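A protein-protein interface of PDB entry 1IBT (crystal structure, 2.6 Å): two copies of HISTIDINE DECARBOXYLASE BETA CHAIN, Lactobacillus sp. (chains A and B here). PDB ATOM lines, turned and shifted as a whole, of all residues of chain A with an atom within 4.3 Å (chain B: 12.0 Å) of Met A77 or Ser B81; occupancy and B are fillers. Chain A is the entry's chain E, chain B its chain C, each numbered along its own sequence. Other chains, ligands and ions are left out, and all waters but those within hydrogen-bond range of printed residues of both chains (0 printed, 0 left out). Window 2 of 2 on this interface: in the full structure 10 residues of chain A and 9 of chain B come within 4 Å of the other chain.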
ATOM      1  N   TYR A  62      39.715  -0.082  13.465  1.00  0.00           N
ATOM      2  CA  TYR A  62      38.731   0.994  13.306  1.00  0.00           C
ATOM      3  C   TYR A  62      37.358   0.583  13.834  1.00  0.00           C
ATOM      4  O   TYR A  62      36.911   1.154  14.837  1.00  0.00           O
ATOM      5  CB  TYR A  62      38.581   1.383  11.833  1.00  0.00           C
ATOM      6  CG  TYR A  62      38.259   2.854  11.767  1.00  0.00           C
ATOM      7  CD1 TYR A  62      39.076   3.738  12.482  1.00  0.00           C
ATOM      8  CD2 TYR A  62      37.159   3.330  11.023  1.00  0.00           C
ATOM      9  CE1 TYR A  62      38.800   5.102  12.459  1.00  0.00           C
ATOM     10  CE2 TYR A  62      36.880   4.710  11.006  1.00  0.00           C
ATOM     11  CZ  TYR A  62      37.712   5.576  11.723  1.00  0.00           C
ATOM     12  OH  TYR A  62      37.502   6.934  11.678  1.00  0.00           O
ATOM     13  N   GLU A  66      34.926   1.988  16.799  1.00  0.00           N
ATOM     14  CA  GLU A  66      33.551   2.416  16.474  1.00  0.00           C
ATOM     15  C   GLU A  66      32.497   1.669  17.313  1.00  0.00           C
ATOM     16  O   GLU A  66      31.536   2.318  17.739  1.00  0.00           O
ATOM     17  CB  GLU A  66      33.209   2.155  14.997  1.00  0.00           C
ATOM     18  CG  GLU A  66      34.099   2.757  13.911  1.00  0.00           C
ATOM     19  CD  GLU A  66      33.465   2.619  12.521  1.00  0.00           C
ATOM     20  OE1 GLU A  66      33.287   3.672  11.880  1.00  0.00           O
ATOM     21  OE2 GLU A  66      33.141   1.486  12.111  1.00  0.00           O
ATOM     22  N   ILE A  72      28.775   3.447  17.168  1.00  0.00           N
ATOM     23  CA  ILE A  72      28.523   4.088  15.900  1.00  0.00           C
ATOM     24  C   ILE A  72      28.945   3.056  14.901  1.00  0.00           C
ATOM     25  O   ILE A  72      29.598   3.362  13.922  1.00  0.00           O
ATOM     26  CB  ILE A  72      29.362   5.385  15.683  1.00  0.00           C
ATOM     27  CG1 ILE A  72      30.841   5.169  15.813  1.00  0.00           C
ATOM     28  CG2 ILE A  72      29.040   6.370  16.742  1.00  0.00           C
ATOM     29  CD1 ILE A  72      31.615   6.125  14.910  1.00  0.00           C
ATOM     30  N   ILE A  75      28.442   2.773  10.015  1.00  0.00           N
ATOM     31  CA  ILE A  75      28.036   4.111   9.668  1.00  0.00           C
ATOM     32  C   ILE A  75      28.843   4.487   8.440  1.00  0.00           C
ATOM     33  O   ILE A  75      29.890   3.887   8.283  1.00  0.00           O
ATOM     34  CB  ILE A  75      28.328   4.845  10.997  1.00  0.00           C
ATOM     35  CG1 ILE A  75      26.978   5.101  11.537  1.00  0.00           C
ATOM     36  CG2 ILE A  75      29.145   6.119  10.944  1.00  0.00           C
ATOM     37  CD1 ILE A  75      26.182   3.831  11.888  1.00  0.00           C
ATOM     38  N   ASN A  76      28.497   5.373   7.511  1.00  0.00           N
ATOM     39  CA  ASN A  76      29.371   5.693   6.388  1.00  0.00           C
ATOM     40  C   ASN A  76      29.932   7.042   6.756  1.00  0.00           C
ATOM     41  O   ASN A  76      29.418   8.109   6.406  1.00  0.00           O
ATOM     42  CB  ASN A  76      28.593   5.787   5.088  1.00  0.00           C
ATOM     43  CG  ASN A  76      28.292   4.452   4.437  1.00  0.00           C
ATOM     44  OD1 ASN A  76      27.588   3.595   4.923  1.00  0.00           O
ATOM     45  ND2 ASN A  76      28.811   4.053   3.301  1.00  0.00           N
ATOM     46  N   MET A  77      31.000   7.007   7.528  1.00  0.00           N
ATOM     47  CA  MET A  77      31.608   8.196   8.068  1.00  0.00           C
ATOM     48  C   MET A  77      32.108   9.129   6.988  1.00  0.00           C
ATOM     49  O   MET A  77      32.763   8.721   6.050  1.00  0.00           O
ATOM     50  CB  MET A  77      32.714   7.717   8.971  1.00  0.00           C
ATOM     51  CG  MET A  77      33.789   8.715   9.405  1.00  0.00           C
ATOM     52  SD  MET A  77      34.101   8.888  11.178  1.00  0.00           S
ATOM     53  CE  MET A  77      33.714   7.223  11.683  1.00  0.00           C
ATOM     54  N   THR A  78      31.798  10.390   7.067  1.00  0.00           N
ATOM     55  CA  THR A  78      32.259  11.342   6.102  1.00  0.00           C
ATOM     56  C   THR A  78      32.987  12.369   6.946  1.00  0.00           C
ATOM     57  O   THR A  78      32.582  12.577   8.087  1.00  0.00           O
ATOM     58  CB  THR A  78      31.030  11.901   5.405  1.00  0.00           C
ATOM     59  OG1 THR A  78      30.201  10.812   4.995  1.00  0.00           O
ATOM     60  CG2 THR A  78      31.444  12.731   4.212  1.00  0.00           C
ATOM     61  N   TYR B  27      23.574  10.507  -3.853  1.00  0.00           N
ATOM     62  CA  TYR B  27      22.725  10.424  -2.699  1.00  0.00           C
ATOM     63  C   TYR B  27      23.005  11.694  -1.931  1.00  0.00           C
ATOM     64  O   TYR B  27      24.133  12.173  -1.911  1.00  0.00           O
ATOM     65  CB  TYR B  27      23.116   9.206  -1.926  1.00  0.00           C
ATOM     66  CG  TYR B  27      22.521   9.065  -0.546  1.00  0.00           C
ATOM     67  CD1 TYR B  27      21.187   8.753  -0.398  1.00  0.00           C
ATOM     68  CD2 TYR B  27      23.308   9.298   0.584  1.00  0.00           C
ATOM     69  CE1 TYR B  27      20.624   8.675   0.868  1.00  0.00           C
ATOM     70  CE2 TYR B  27      22.735   9.229   1.856  1.00  0.00           C
ATOM     71  CZ  TYR B  27      21.393   8.918   1.983  1.00  0.00           C
ATOM     72  OH  TYR B  27      20.783   8.900   3.206  1.00  0.00           O
ATOM     73  N   MET B  28      21.923  12.199  -1.329  1.00  0.00           N
ATOM     74  CA  MET B  28      21.830  13.454  -0.609  1.00  0.00           C
ATOM     75  C   MET B  28      21.767  14.694  -1.470  1.00  0.00           C
ATOM     76  O   MET B  28      21.557  15.778  -0.937  1.00  0.00           O
ATOM     77  CB  MET B  28      22.988  13.625   0.356  1.00  0.00           C
ATOM     78  CG  MET B  28      22.913  12.623   1.493  1.00  0.00           C
ATOM     79  SD  MET B  28      24.122  12.861   2.787  1.00  0.00           S
ATOM     80  CE  MET B  28      25.514  12.193   1.941  1.00  0.00           C
ATOM     81  N   TYR B  37      19.297   5.004  -1.337  1.00  0.00           N
ATOM     82  CA  TYR B  37      20.396   5.077  -2.267  1.00  0.00           C
ATOM     83  C   TYR B  37      20.672   3.769  -2.976  1.00  0.00           C
ATOM     84  O   TYR B  37      20.329   2.694  -2.481  1.00  0.00           O
ATOM     85  CB  TYR B  37      21.666   5.523  -1.550  1.00  0.00           C
ATOM     86  CG  TYR B  37      22.129   4.720  -0.338  1.00  0.00           C
ATOM     87  CD1 TYR B  37      22.637   3.427  -0.451  1.00  0.00           C
ATOM     88  CD2 TYR B  37      22.060   5.301   0.917  1.00  0.00           C
ATOM     89  CE1 TYR B  37      23.065   2.725   0.671  1.00  0.00           C
ATOM     90  CE2 TYR B  37      22.495   4.608   2.037  1.00  0.00           C
ATOM     91  CZ  TYR B  37      22.992   3.332   1.907  1.00  0.00           C
ATOM     92  OH  TYR B  37      23.433   2.662   3.025  1.00  0.00           O
ATOM     93  N   THR B  39      23.933   1.649  -4.923  1.00  0.00           N
ATOM     94  CA  THR B  39      25.374   1.611  -4.999  1.00  0.00           C
ATOM     95  C   THR B  39      25.808   0.513  -5.958  1.00  0.00           C
ATOM     96  O   THR B  39      24.990  -0.295  -6.405  1.00  0.00           O
ATOM     97  CB  THR B  39      25.902   1.396  -3.568  1.00  0.00           C
ATOM     98  OG1 THR B  39      27.287   1.610  -3.678  1.00  0.00           O
ATOM     99  CG2 THR B  39      25.606   0.025  -2.956  1.00  0.00           C
ATOM    100  N   MET B  77      33.808  13.717  -6.287  1.00  0.00           N
ATOM    101  CA  MET B  77      33.890  12.598  -5.376  1.00  0.00           C
ATOM    102  C   MET B  77      34.045  13.028  -3.935  1.00  0.00           C
ATOM    103  O   MET B  77      34.851  13.882  -3.619  1.00  0.00           O
ATOM    104  CB  MET B  77      35.058  11.758  -5.841  1.00  0.00           C
ATOM    105  CG  MET B  77      35.626  10.735  -4.881  1.00  0.00           C
ATOM    106  SD  MET B  77      35.724   9.080  -5.607  1.00  0.00           S
ATOM    107  CE  MET B  77      35.971   9.353  -7.325  1.00  0.00           C
ATOM    108  N   THR B  78      33.253  12.501  -3.047  1.00  0.00           N
ATOM    109  CA  THR B  78      33.356  12.848  -1.661  1.00  0.00           C
ATOM    110  C   THR B  78      33.572  11.501  -0.988  1.00  0.00           C
ATOM    111  O   THR B  78      33.070  10.496  -1.513  1.00  0.00           O
ATOM    112  CB  THR B  78      32.072  13.499  -1.268  1.00  0.00           C
ATOM    113  OG1 THR B  78      31.768  14.540  -2.192  1.00  0.00           O
ATOM    114  CG2 THR B  78      32.204  14.062   0.123  1.00  0.00           C
ATOM    115  N   THR B  79      34.283  11.378   0.141  1.00  0.00           N
ATOM    116  CA  THR B  79      34.628  10.050   0.649  1.00  0.00           C
ATOM    117  C   THR B  79      33.929   9.711   1.953  1.00  0.00           C
ATOM    118  O   THR B  79      33.756  10.554   2.845  1.00  0.00           O
ATOM    119  CB  THR B  79      36.154   9.983   0.830  1.00  0.00           C
ATOM    120  OG1 THR B  79      36.689  10.386  -0.409  1.00  0.00           O
ATOM    121  CG2 THR B  79      36.685   8.614   1.213  1.00  0.00           C
ATOM    122  N   ALA B  80      33.535   8.463   2.022  1.00  0.00           N
ATOM    123  CA  ALA B  80      32.944   7.909   3.210  1.00  0.00           C
ATOM    124  C   ALA B  80      33.779   6.695   3.555  1.00  0.00           C
ATOM    125  O   ALA B  80      34.292   6.033   2.649  1.00  0.00           O
ATOM    126  CB  ALA B  80      31.548   7.441   2.956  1.00  0.00           C
ATOM    127  N   SER B  81      33.889   6.363   4.827  1.00  0.00           N
ATOM    128  CA  SER B  81      34.749   5.285   5.286  1.00  0.00           C
ATOM    129  C   SER B  81      34.318   4.982   6.725  1.00  0.00           C
ATOM    130  O   SER B  81      33.233   4.445   6.909  1.00  0.00           O
ATOM    131  CB  SER B  81      36.231   5.800   5.153  1.00  0.00           C
ATOM    132  OG  SER B  81      36.436   7.085   5.776  1.00  0.00           O
ATOM    133  OXT SER B  81      35.015   5.378   7.656  1.00  0.00           O
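Positions printed for both chains: 77 and 78.
Of the 9 printed residues of chain B, 3 touch a printed residue of chain A. Hydrophobic or aromatic side chains of chain B within 4 Å of the printed part of chain A: Ala B80. Of the 7 printed residues of chain A, 4 touch a printed residue of chain B. Hydrophobic or aromatic side chains of chain A that line the printed part of chain B: Tyr A62 and Met A77.
Met A77 touches just these residues of chain B: Thr B79 (3.8 Å), Ala B80 (3.0 Å) and Ser B81 (2.9 Å). Ser B81 touches just these residues of chain A: Tyr A62 (3.9 Å), Ile A75 (3.7 Å) and Met A77 (2.9 Å). Ile A75 touches just one residue of chain B: Ser B81. Of the printed residues of chain B, Thr A78 touches Thr B79 (3.5 Å). Printed residues of chain B within 4 Å of Tyr A62: Ser B81. Of the printed residues of chain A, Ala B80 touches Met A77 (3.0 Å). Thr B78 touches none of the printed residues of chain A. The nearest residue of chain B that does not touch Met A77 is Thr B78 (7.6 Å).
The backbone NH of Ser B81 sits at hydrogen-bond distance from the backbone carbonyl oxygen of Met A77, 2.9 Å away.
Among the printed residues, pairs that only touch across the chains: Tyr A62 with Ser B81, Ile A75 with Ser B81, Met A77 with Thr B79, Met A77 with Ala B80 and Thr A78 with Thr B79.
The side-chain hydroxyl of Thr A78 lies within hydrogen-bond range of the backbone carbonyl oxygen of Asn A76, 3.1 Å away.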
